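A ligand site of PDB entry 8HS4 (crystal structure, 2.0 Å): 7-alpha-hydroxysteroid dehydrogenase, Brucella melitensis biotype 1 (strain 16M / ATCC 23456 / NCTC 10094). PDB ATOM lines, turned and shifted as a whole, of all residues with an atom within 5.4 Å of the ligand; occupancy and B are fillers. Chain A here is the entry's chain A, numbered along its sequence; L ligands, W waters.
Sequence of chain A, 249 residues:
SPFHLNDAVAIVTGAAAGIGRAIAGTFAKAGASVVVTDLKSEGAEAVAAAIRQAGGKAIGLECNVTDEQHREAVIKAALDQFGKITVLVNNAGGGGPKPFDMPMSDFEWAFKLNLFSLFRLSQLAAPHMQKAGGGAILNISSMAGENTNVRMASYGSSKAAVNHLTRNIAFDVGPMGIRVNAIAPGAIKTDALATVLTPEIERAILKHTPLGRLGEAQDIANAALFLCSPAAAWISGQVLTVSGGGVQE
A nitrogen (N4) of the ligand lies close to the backbone carbonyl oxygen of Cys 63 (3.3 Å). The backbone carbonyl oxygen (O) of Pro 185 lies close to an oxygen (O14) of the ligand (2.9 Å). Residues that only touch the ligand: Ile 140, Gly 14, Leu 113, Ser 141, Gly 93, Gly 186, Ala 16, Ala 92, Met 143, Ala 17, Gly 18 and Gly 94. Hydrophobic or aromatic side chains within 4 Å of the ligand: Ala 16, Ile 19, Leu 39, Val 65, Ala 92, Leu 113, Ile 140, Tyr 155 and Pro 185. The nearest printed residue that does not touch the ligand is Lys 40 (4.2 Å).
Water W5 lies within hydrogen-bond range of O4 of the ligand (2.8 Å) and O of Gly 93 (2.9 Å). Water W3 lies within hydrogen-bond range of the backbone carbonyl oxygen (O) of Cys 63 (2.9 Å), the backbone NH (N) of Gly 14 (3.1 Å) and the backbone NH (N) of Asp 38 (3.3 Å).
The backbone carbonyl oxygen of Asn 91 is in hydrogen-bond range of an oxygen (O12) of the ligand (2.8 Å). The side-chain amino group (NZ) of Lys 159 is in hydrogen-bond range of an oxygen (O13) of the ligand (2.8 Å). OD1 of Asn 64 sits at hydrogen-bond distance from N3 of the ligand, at 3.2 Å. An oxygen (O6) of the ligand sits at hydrogen-bond distance from the side-chain carboxylate (OD2) of Asp 38 (2.6 Å). N of Leu 39 lies within hydrogen-bond range of N5 of the ligand. The backbone NH (N) of Val 65 sits at hydrogen-bond distance from a nitrogen (N4) of the ligand (3.0 Å). OH of Tyr 155 sits at hydrogen-bond distance from N7 of the ligand (2.7 Å). The backbone NH (N) of Ile 19 sits at hydrogen-bond distance from an oxygen (O9) of the ligand (3.4 Å). The side-chain hydroxyl of Ser 142 sits at hydrogen-bond distance from a nitrogen (N7) of the ligand (2.7 Å). A nitrogen (N7) of the ligand is in hydrogen-bond range of the side-chain carboxylate (OE2) of Glu 249, 2.8 Å away.
The side-chain hydroxyl of Ser 142 lies within hydrogen-bond range of the side-chain carboxylate of Glu 249. N of Ala 92 lies within hydrogen-bond range of OG1 of Thr 13 (3.0 Å). The side-chain amide nitrogen (ND2) of Asn 91 lies close to the backbone NH (N) of Gly 20, at 3.4 Å. The backbone NH (N) of Cys 63 sits at hydrogen-bond distance from the backbone carbonyl oxygen (O) of Asp 38 (2.7 Å). The side-chain amino group (NZ) of Lys 159 sits at hydrogen-bond distance from the backbone carbonyl oxygen (O) of Ile 140 (3.4 Å). The backbone NH (N) of Ala 15 sits at hydrogen-bond distance from the side-chain carboxylate (OD1) of Asp 38. The backbone NH (N) of Ala 16 lies within hydrogen-bond range of the side-chain carboxylate (OD1) of Asp 38, at 3.0 Å. OG1 of Thr 66 is in hydrogen-bond range of OD1 of Asn 64, 2.7 Å away.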
ATOM      1  N   THR A  13      -1.701  23.500 -10.107  1.00  0.00           N
ATOM      2  CA  THR A  13      -1.218  22.871  -8.870  1.00  0.00           C
ATOM      3  C   THR A  13      -2.300  21.996  -8.254  1.00  0.00           C
ATOM      4  O   THR A  13      -3.500  22.146  -8.533  1.00  0.00           O
ATOM      5  CB  THR A  13      -0.739  23.906  -7.853  1.00  0.00           C
ATOM      6  OG1 THR A  13      -1.837  24.745  -7.457  1.00  0.00           O
ATOM      7  CG2 THR A  13       0.382  24.766  -8.442  1.00  0.00           C
ATOM      8  N   GLY A  14      -1.862  21.080  -7.387  1.00  0.00           N
ATOM      9  CA  GLY A  14      -2.796  20.127  -6.786  1.00  0.00           C
ATOM     10  C   GLY A  14      -3.611  19.366  -7.810  1.00  0.00           C
ATOM     11  O   GLY A  14      -4.805  19.128  -7.603  1.00  0.00           O
ATOM     12  N   ALA A  15      -2.973  18.958  -8.904  1.00  0.00           N
ATOM     13  CA  ALA A  15      -3.729  18.496 -10.067  1.00  0.00           C
ATOM     14  C   ALA A  15      -3.805  16.972 -10.174  1.00  0.00           C
ATOM     15  O   ALA A  15      -4.242  16.467 -11.216  1.00  0.00           O
ATOM     16  CB  ALA A  15      -3.133  19.088 -11.335  1.00  0.00           C
ATOM     17  N   ALA A  16      -3.441  16.234  -9.127  1.00  0.00           N
ATOM     18  CA  ALA A  16      -3.495  14.778  -9.261  1.00  0.00           C
ATOM     19  C   ALA A  16      -4.895  14.216  -9.074  1.00  0.00           C
ATOM     20  O   ALA A  16      -5.146  13.070  -9.481  1.00  0.00           O
ATOM     21  CB  ALA A  16      -2.559  14.114  -8.258  1.00  0.00           C
ATOM     22  N   ALA A  17      -5.827  14.987  -8.511  1.00  0.00           N
ATOM     23  CA  ALA A  17      -7.150  14.456  -8.237  1.00  0.00           C
ATOM     24  C   ALA A  17      -8.143  15.613  -8.193  1.00  0.00           C
ATOM     25  O   ALA A  17      -7.766  16.784  -8.166  1.00  0.00           O
ATOM     26  CB  ALA A  17      -7.183  13.658  -6.920  1.00  0.00           C
ATOM     27  N   GLY A  18      -9.435  15.254  -8.211  1.00  0.00           N
ATOM     28  CA  GLY A  18     -10.513  16.198  -7.959  1.00  0.00           C
ATOM     29  C   GLY A  18     -10.550  17.366  -8.936  1.00  0.00           C
ATOM     30  O   GLY A  18     -10.381  17.199 -10.157  1.00  0.00           O
ATOM     31  N   ILE A  19     -10.765  18.555  -8.384  1.00  0.00           N
ATOM     32  CA  ILE A  19     -10.900  19.777  -9.179  1.00  0.00           C
ATOM     33  C   ILE A  19      -9.649  20.012 -10.020  1.00  0.00           C
ATOM     34  O   ILE A  19      -9.740  20.275 -11.226  1.00  0.00           O
ATOM     35  CB  ILE A  19     -11.203  20.976  -8.269  1.00  0.00           C
ATOM     36  CG1 ILE A  19     -12.622  20.881  -7.698  1.00  0.00           C
ATOM     37  CG2 ILE A  19     -11.016  22.288  -9.000  1.00  0.00           C
ATOM     38  CD1 ILE A  19     -12.859  21.822  -6.501  1.00  0.00           C
ATOM     39  N   GLY A  20      -8.465  19.916  -9.413  1.00  0.00           N
ATOM     40  CA  GLY A  20      -7.248  20.222 -10.137  1.00  0.00           C
ATOM     41  C   GLY A  20      -7.006  19.270 -11.299  1.00  0.00           C
ATOM     42  O   GLY A  20      -6.566  19.699 -12.372  1.00  0.00           O
ATOM     43  N   ASP A  38       1.665  18.309  -8.468  1.00  0.00           N
ATOM     44  CA  ASP A  38       0.984  17.828  -7.261  1.00  0.00           C
ATOM     45  C   ASP A  38       2.014  17.556  -6.189  1.00  0.00           C
ATOM     46  O   ASP A  38       3.191  17.313  -6.474  1.00  0.00           O
ATOM     47  CB  ASP A  38       0.173  16.553  -7.531  1.00  0.00           C
ATOM     48  CG  ASP A  38      -0.878  16.319  -6.468  1.00  0.00           C
ATOM     49  OD1 ASP A  38      -1.996  16.850  -6.623  1.00  0.00           O
ATOM     50  OD2 ASP A  38      -0.592  15.604  -5.469  1.00  0.00           O
ATOM     51  N   LEU A  39       1.562  17.593  -4.938  1.00  0.00           N
ATOM     52  CA  LEU A  39       2.388  17.123  -3.832  1.00  0.00           C
ATOM     53  C   LEU A  39       2.941  15.735  -4.107  1.00  0.00           C
ATOM     54  O   LEU A  39       4.111  15.444  -3.831  1.00  0.00           O
ATOM     55  CB  LEU A  39       1.574  17.125  -2.533  1.00  0.00           C
ATOM     56  CG  LEU A  39       2.309  16.670  -1.281  1.00  0.00           C
ATOM     57  CD1 LEU A  39       3.389  17.677  -0.906  1.00  0.00           C
ATOM     58  CD2 LEU A  39       1.316  16.463  -0.136  1.00  0.00           C
ATOM     59  N   LYS A  40       2.110  14.857  -4.680  1.00  0.00           N
ATOM     60  CA  LYS A  40       2.477  13.475  -4.931  1.00  0.00           C
ATOM     61  C   LYS A  40       3.018  13.367  -6.354  1.00  0.00           C
ATOM     62  O   LYS A  40       2.268  13.595  -7.321  1.00  0.00           O
ATOM     63  CB  LYS A  40       1.272  12.558  -4.734  1.00  0.00           C
ATOM     64  CG  LYS A  40       0.736  12.506  -3.311  1.00  0.00           C
ATOM     65  CD  LYS A  40       1.857  12.229  -2.302  1.00  0.00           C
ATOM     66  CE  LYS A  40       2.338  10.783  -2.396  1.00  0.00           C
ATOM     67  NZ  LYS A  40       3.838  10.679  -2.315  1.00  0.00           N
ATOM     68  N   CYS A  63       5.337  18.933  -6.884  1.00  0.00           N
ATOM     69  CA  CYS A  63       5.469  20.308  -6.377  1.00  0.00           C
ATOM     70  C   CYS A  63       4.660  20.446  -5.095  1.00  0.00           C
ATOM     71  O   CYS A  63       3.423  20.476  -5.147  1.00  0.00           O
ATOM     72  CB  CYS A  63       5.042  21.344  -7.403  1.00  0.00           C
ATOM     73  SG  CYS A  63       5.110  23.072  -6.747  1.00  0.00           S
ATOM     74  N   ASN A  64       5.362  20.494  -3.969  1.00  0.00           N
ATOM     75  CA  ASN A  64       4.810  21.015  -2.728  1.00  0.00           C
ATOM     76  C   ASN A  64       4.785  22.528  -2.847  1.00  0.00           C
ATOM     77  O   ASN A  64       5.848  23.159  -2.831  1.00  0.00           O
ATOM     78  CB  ASN A  64       5.676  20.540  -1.564  1.00  0.00           C
ATOM     79  CG  ASN A  64       5.237  21.123  -0.231  1.00  0.00           C
ATOM     80  OD1 ASN A  64       4.249  21.856  -0.155  1.00  0.00           O
ATOM     81  ND2 ASN A  64       5.977  20.798   0.827  1.00  0.00           N
ATOM     82  N   VAL A  65       3.597  23.138  -2.958  1.00  0.00           N
ATOM     83  CA  VAL A  65       3.525  24.566  -3.241  1.00  0.00           C
ATOM     84  C   VAL A  65       4.079  25.437  -2.115  1.00  0.00           C
ATOM     85  O   VAL A  65       4.365  26.626  -2.345  1.00  0.00           O
ATOM     86  CB  VAL A  65       2.087  25.039  -3.587  1.00  0.00           C
ATOM     87  CG1 VAL A  65       1.589  24.333  -4.847  1.00  0.00           C
ATOM     88  CG2 VAL A  65       1.098  24.836  -2.418  1.00  0.00           C
ATOM     89  N   THR A  66       4.280  24.886  -0.919  1.00  0.00           N
ATOM     90  CA  THR A  66       4.855  25.614   0.214  1.00  0.00           C
ATOM     91  C   THR A  66       6.384  25.567   0.253  1.00  0.00           C
ATOM     92  O   THR A  66       6.979  26.075   1.202  1.00  0.00           O
ATOM     93  CB  THR A  66       4.278  25.072   1.531  1.00  0.00           C
ATOM     94  OG1 THR A  66       4.680  23.703   1.699  1.00  0.00           O
ATOM     95  CG2 THR A  66       2.747  25.135   1.531  1.00  0.00           C
ATOM     96  N   ASN A  90      -3.960  28.164  -9.285  1.00  0.00           N
ATOM     97  CA  ASN A  90      -3.521  27.874  -7.921  1.00  0.00           C
ATOM     98  C   ASN A  90      -4.636  27.078  -7.245  1.00  0.00           C
ATOM     99  O   ASN A  90      -5.533  27.628  -6.615  1.00  0.00           O
ATOM    100  CB  ASN A  90      -3.228  29.171  -7.177  1.00  0.00           C
ATOM    101  CG  ASN A  90      -2.008  29.881  -7.723  1.00  0.00           C
ATOM    102  OD1 ASN A  90      -0.924  29.303  -7.781  1.00  0.00           O
ATOM    103  ND2 ASN A  90      -2.179  31.139  -8.094  1.00  0.00           N
ATOM    104  N   ASN A  91      -4.581  25.764  -7.398  1.00  0.00           N
ATOM    105  CA  ASN A  91      -5.618  24.903  -6.851  1.00  0.00           C
ATOM    106  C   ASN A  91      -5.188  24.223  -5.561  1.00  0.00           C
ATOM    107  O   ASN A  91      -6.048  23.936  -4.720  1.00  0.00           O
ATOM    108  CB  ASN A  91      -6.023  23.863  -7.913  1.00  0.00           C
ATOM    109  CG  ASN A  91      -6.939  22.798  -7.366  1.00  0.00           C
ATOM    110  OD1 ASN A  91      -8.099  23.061  -7.038  1.00  0.00           O
ATOM    111  ND2 ASN A  91      -6.413  21.569  -7.236  1.00  0.00           N
ATOM    112  N   ALA A  92      -3.899  23.996  -5.360  1.00  0.00           N
ATOM    113  CA  ALA A  92      -3.425  23.399  -4.112  1.00  0.00           C
ATOM    114  C   ALA A  92      -3.822  24.271  -2.929  1.00  0.00           C
ATOM    115  O   ALA A  92      -3.667  25.494  -2.951  1.00  0.00           O
ATOM    116  CB  ALA A  92      -1.901  23.221  -4.149  1.00  0.00           C
ATOM    117  N   GLY A  93      -4.347  23.619  -1.900  1.00  0.00           N
ATOM    118  CA  GLY A  93      -4.778  24.287  -0.689  1.00  0.00           C
ATOM    119  C   GLY A  93      -5.337  23.213   0.226  1.00  0.00           C
ATOM    120  O   GLY A  93      -5.263  22.021  -0.083  1.00  0.00           O
ATOM    121  N   GLY A  94      -5.907  23.621   1.348  1.00  0.00           N
ATOM    122  CA  GLY A  94      -6.409  22.633   2.290  1.00  0.00           C
ATOM    123  C   GLY A  94      -6.716  23.262   3.643  1.00  0.00           C
ATOM    124  O   GLY A  94      -6.646  24.473   3.815  1.00  0.00           O
ATOM    125  N   LEU A 113      -0.111  27.529   3.536  1.00  0.00           N
ATOM    126  CA  LEU A 113      -0.619  26.610   2.527  1.00  0.00           C
ATOM    127  C   LEU A 113      -1.593  27.286   1.577  1.00  0.00           C
ATOM    128  O   LEU A 113      -1.472  27.159   0.347  1.00  0.00           O
ATOM    129  CB  LEU A 113      -1.261  25.399   3.210  1.00  0.00           C
ATOM    130  CG  LEU A 113      -1.956  24.383   2.286  1.00  0.00           C
ATOM    131  CD1 LEU A 113      -0.924  23.773   1.326  1.00  0.00           C
ATOM    132  CD2 LEU A 113      -2.657  23.301   3.099  1.00  0.00           C
ATOM    133  N   ASN A 114      -2.572  28.011   2.115  1.00  0.00           N
ATOM    134  CA  ASN A 114      -3.632  28.548   1.269  1.00  0.00           C
ATOM    135  C   ASN A 114      -3.288  29.902   0.635  1.00  0.00           C
ATOM    136  O   ASN A 114      -3.867  30.245  -0.410  1.00  0.00           O
ATOM    137  CB  ASN A 114      -4.931  28.695   2.076  1.00  0.00           C
ATOM    138  CG  ASN A 114      -5.589  27.338   2.392  1.00  0.00           C
ATOM    139  OD1 ASN A 114      -5.555  26.415   1.591  1.00  0.00           O
ATOM    140  ND2 ASN A 114      -6.217  27.242   3.578  1.00  0.00           N
ATOM    141  N   ILE A 140      -8.231  28.937  -6.589  1.00  0.00           N
ATOM    142  CA  ILE A 140      -9.354  28.152  -6.066  1.00  0.00           C
ATOM    143  C   ILE A 140      -9.460  28.464  -4.587  1.00  0.00           C
ATOM    144  O   ILE A 140      -8.599  28.066  -3.790  1.00  0.00           O
ATOM    145  CB  ILE A 140      -9.180  26.655  -6.325  1.00  0.00           C
ATOM    146  CG1 ILE A 140      -8.873  26.390  -7.808  1.00  0.00           C
ATOM    147  CG2 ILE A 140     -10.434  25.917  -5.915  1.00  0.00           C
ATOM    148  CD1 ILE A 140      -9.980  26.886  -8.773  1.00  0.00           C
ATOM    149  N   SER A 141     -10.505  29.187  -4.216  1.00  0.00           N
ATOM    150  CA  SER A 141     -10.738  29.612  -2.843  1.00  0.00           C
ATOM    151  C   SER A 141     -11.616  28.598  -2.111  1.00  0.00           C
ATOM    152  O   SER A 141     -11.394  27.390  -2.182  1.00  0.00           O
ATOM    153  CB  SER A 141     -11.385  30.997  -2.836  1.00  0.00           C
ATOM    154  OG  SER A 141     -11.277  31.599  -1.569  1.00  0.00           O
ATOM    155  N   SER A 142     -12.636  29.087  -1.435  1.00  0.00           N
ATOM    156  CA  SER A 142     -13.573  28.242  -0.704  1.00  0.00           C
ATOM    157  C   SER A 142     -14.758  29.111  -0.327  1.00  0.00           C
ATOM    158  O   SER A 142     -14.598  30.313  -0.124  1.00  0.00           O
ATOM    159  CB  SER A 142     -12.918  27.633   0.547  1.00  0.00           C
ATOM    160  OG  SER A 142     -13.882  27.097   1.447  1.00  0.00           O
ATOM    161  N   MET A 143     -15.935  28.503  -0.236  1.00  0.00           N
ATOM    162  CA  MET A 143     -17.087  29.256   0.251  1.00  0.00           C
ATOM    163  C   MET A 143     -16.896  29.723   1.700  1.00  0.00           C
ATOM    164  O   MET A 143     -17.562  30.662   2.133  1.00  0.00           O
ATOM    165  CB  MET A 143     -18.373  28.453   0.101  1.00  0.00           C
ATOM    166  CG  MET A 143     -18.837  28.289  -1.337  1.00  0.00           C
ATOM    167  SD  MET A 143     -20.286  27.221  -1.429  1.00  0.00           S
ATOM    168  CE  MET A 143     -21.523  28.420  -0.971  1.00  0.00           C
ATOM    169  N   ALA A 144     -16.008  29.073   2.454  1.00  0.00           N
ATOM    170  CA  ALA A 144     -15.709  29.545   3.801  1.00  0.00           C
ATOM    171  C   ALA A 144     -15.151  30.959   3.805  1.00  0.00           C
ATOM    172  O   ALA A 144     -15.227  31.640   4.840  1.00  0.00           O
ATOM    173  CB  ALA A 144     -14.729  28.577   4.471  1.00  0.00           C
ATOM    174  N   TYR A 155      -9.329  28.372   8.681  1.00  0.00           N
ATOM    175  CA  TYR A 155      -9.728  28.030   7.318  1.00  0.00           C
ATOM    176  C   TYR A 155     -10.520  29.171   6.665  1.00  0.00           C
ATOM    177  O   TYR A 155     -10.252  29.550   5.521  1.00  0.00           O
ATOM    178  CB  TYR A 155     -10.539  26.740   7.331  1.00  0.00           C
ATOM    179  CG  TYR A 155     -10.847  26.212   5.943  1.00  0.00           C
ATOM    180  CD1 TYR A 155      -9.824  25.789   5.104  1.00  0.00           C
ATOM    181  CD2 TYR A 155     -12.154  26.145   5.479  1.00  0.00           C
ATOM    182  CE1 TYR A 155     -10.089  25.315   3.837  1.00  0.00           C
ATOM    183  CE2 TYR A 155     -12.438  25.667   4.208  1.00  0.00           C
ATOM    184  CZ  TYR A 155     -11.389  25.248   3.389  1.00  0.00           C
ATOM    185  OH  TYR A 155     -11.626  24.781   2.129  1.00  0.00           O
ATOM    186  N   LYS A 159      -8.898  31.585   3.606  1.00  0.00           N
ATOM    187  CA  LYS A 159      -9.541  31.607   2.299  1.00  0.00           C
ATOM    188  C   LYS A 159     -10.150  32.971   1.987  1.00  0.00           C
ATOM    189  O   LYS A 159     -10.178  33.379   0.820  1.00  0.00           O
ATOM    190  CB  LYS A 159     -10.596  30.500   2.226  1.00  0.00           C
ATOM    191  CG  LYS A 159     -10.023  29.066   2.225  1.00  0.00           C
ATOM    192  CD  LYS A 159      -9.268  28.758   0.938  1.00  0.00           C
ATOM    193  CE  LYS A 159      -8.887  27.275   0.817  1.00  0.00           C
ATOM    194  NZ  LYS A 159      -8.413  26.950  -0.557  1.00  0.00           N
ATOM    195  N   PRO A 185     -15.515  26.954  -4.725  1.00  0.00           N
ATOM    196  CA  PRO A 185     -16.308  25.769  -5.026  1.00  0.00           C
ATOM    197  C   PRO A 185     -17.205  25.372  -3.875  1.00  0.00           C
ATOM    198  O   PRO A 185     -16.871  25.553  -2.708  1.00  0.00           O
ATOM    199  CB  PRO A 185     -15.249  24.689  -5.291  1.00  0.00           C
ATOM    200  CG  PRO A 185     -14.048  25.136  -4.572  1.00  0.00           C
ATOM    201  CD  PRO A 185     -14.097  26.629  -4.481  1.00  0.00           C
ATOM    202  N   GLY A 186     -18.380  24.838  -4.224  1.00  0.00           N
ATOM    203  CA  GLY A 186     -19.310  24.335  -3.232  1.00  0.00           C
ATOM    204  C   GLY A 186     -18.936  22.935  -2.782  1.00  0.00           C
ATOM    205  O   GLY A 186     -17.758  22.642  -2.578  1.00  0.00           O
ATOM    206  N   ILE A 188     -18.425  19.360  -3.865  1.00  0.00           N
ATOM    207  CA  ILE A 188     -18.180  18.576  -5.069  1.00  0.00           C
ATOM    208  C   ILE A 188     -17.892  17.148  -4.633  1.00  0.00           C
ATOM    209  O   ILE A 188     -17.046  16.920  -3.757  1.00  0.00           O
ATOM    210  CB  ILE A 188     -17.013  19.155  -5.891  1.00  0.00           C
ATOM    211  CG1 ILE A 188     -17.428  20.482  -6.539  1.00  0.00           C
ATOM    212  CG2 ILE A 188     -16.567  18.160  -6.941  1.00  0.00           C
ATOM    213  CD1 ILE A 188     -17.197  21.694  -5.669  1.00  0.00           C
ATOM    214  N   GLU A 249     -21.621  26.923   3.608  1.00  0.00           N
ATOM    215  CA  GLU A 249     -20.405  26.159   3.439  1.00  0.00           C
ATOM    216  C   GLU A 249     -20.593  24.761   4.037  1.00  0.00           C
ATOM    217  O   GLU A 249     -21.397  24.575   4.944  1.00  0.00           O
ATOM    218  CB  GLU A 249     -19.228  26.909   4.100  1.00  0.00           C
ATOM    219  CG  GLU A 249     -18.013  26.038   4.394  1.00  0.00           C
ATOM    220  CD  GLU A 249     -17.194  25.682   3.155  1.00  0.00           C
ATOM    221  OE1 GLU A 249     -17.637  25.924   2.030  1.00  0.00           O
ATOM    222  OE2 GLU A 249     -16.092  25.151   3.329  1.00  0.00           O
HETATM  223  P1  LIG L   1      -8.475  16.916  -3.301  1.00  0.00           P
HETATM  224  O1  LIG L   1      -8.097  16.293  -1.981  1.00  0.00           O
HETATM  225  O2  LIG L   1      -9.547  16.332  -4.167  1.00  0.00           O
HETATM  226  O3  LIG L   1      -7.139  17.045  -4.174  1.00  0.00           O
HETATM  227  C1  LIG L   1      -6.143  17.957  -3.753  1.00  0.00           C
HETATM  228  C2  LIG L   1      -4.849  17.665  -4.486  1.00  0.00           C
HETATM  229  O4  LIG L   1      -3.895  18.652  -4.095  1.00  0.00           O
HETATM  230  C3  LIG L   1      -4.292  16.315  -4.101  1.00  0.00           C
HETATM  231  O5  LIG L   1      -3.887  15.603  -5.253  1.00  0.00           O
HETATM  232  C4  LIG L   1      -3.126  16.632  -3.200  1.00  0.00           C
HETATM  233  O6  LIG L   1      -2.072  15.684  -3.303  1.00  0.00           O
HETATM  234  C5  LIG L   1      -2.705  18.002  -3.685  1.00  0.00           C
HETATM  235  N1  LIG L   1      -1.991  18.755  -2.630  1.00  0.00           N
HETATM  236  C6  LIG L   1      -2.250  18.761  -1.318  1.00  0.00           C
HETATM  237  N2  LIG L   1      -1.370  19.566  -0.660  1.00  0.00           N
HETATM  238  C7  LIG L   1      -0.532  20.071  -1.576  1.00  0.00           C
HETATM  239  C8  LIG L   1       0.635  20.980  -1.561  1.00  0.00           C
HETATM  240  N3  LIG L   1       1.093  21.521  -0.420  1.00  0.00           N
HETATM  241  N4  LIG L   1       1.225  21.235  -2.746  1.00  0.00           N
HETATM  242  C9  LIG L   1       0.774  20.701  -3.877  1.00  0.00           C
HETATM  243  N5  LIG L   1      -0.275  19.872  -3.979  1.00  0.00           N
HETATM  244  C10 LIG L   1      -0.954  19.531  -2.871  1.00  0.00           C
HETATM  245  O7  LIG L   1      -8.756  18.470  -2.958  1.00  0.00           O
HETATM  246  P2  LIG L   1      -9.944  19.334  -3.585  1.00  0.00           P
HETATM  247  O8  LIG L   1     -11.148  19.110  -2.732  1.00  0.00           O
HETATM  248  O9  LIG L   1     -10.041  19.132  -5.069  1.00  0.00           O
HETATM  249  O10 LIG L   1      -9.401  20.821  -3.277  1.00  0.00           O
HETATM  250  C11 LIG L   1      -8.817  21.646  -4.277  1.00  0.00           C
HETATM  251  C12 LIG L   1      -8.968  23.121  -3.915  1.00  0.00           C
HETATM  252  O11 LIG L   1     -10.348  23.476  -3.817  1.00  0.00           O
HETATM  253  C13 LIG L   1      -8.346  23.480  -2.578  1.00  0.00           C
HETATM  254  O12 LIG L   1      -7.742  24.768  -2.647  1.00  0.00           O
HETATM  255  C14 LIG L   1      -9.519  23.480  -1.628  1.00  0.00           C
HETATM  256  O13 LIG L   1      -9.305  24.304  -0.489  1.00  0.00           O
HETATM  257  C15 LIG L   1     -10.652  23.966  -2.519  1.00  0.00           C
HETATM  258  N6  LIG L   1     -11.939  23.420  -2.116  1.00  0.00           N
HETATM  259  C16 LIG L   1     -12.673  24.079  -1.214  1.00  0.00           C
HETATM  260  C17 LIG L   1     -13.913  23.576  -0.823  1.00  0.00           C
HETATM  261  C18 LIG L   1     -14.725  24.301   0.208  1.00  0.00           C
HETATM  262  O14 LIG L   1     -15.804  24.801  -0.077  1.00  0.00           O
HETATM  263  N7  LIG L   1     -14.224  24.385   1.434  1.00  0.00           N
HETATM  264  C19 LIG L   1     -14.376  22.401  -1.373  1.00  0.00           C
HETATM  265  C20 LIG L   1     -13.602  21.742  -2.311  1.00  0.00           C
HETATM  266  C21 LIG L   1     -12.368  22.283  -2.666  1.00  0.00           C
HETATM  267  O   HOH W   1      -5.731  27.102  -3.580  1.00  0.00           O
HETATM  268  O   HOH W   2      -7.906  19.064  -6.592  1.00  0.00           O
HETATM  269  O   HOH W   3       1.221  21.164  -6.882  1.00  0.00           O
HETATM  270  O   HOH W   4      -3.377  12.774  -4.880  1.00  0.00           O
HETATM  271  O   HOH W   5      -5.154  20.660  -2.686  1.00  0.00           O
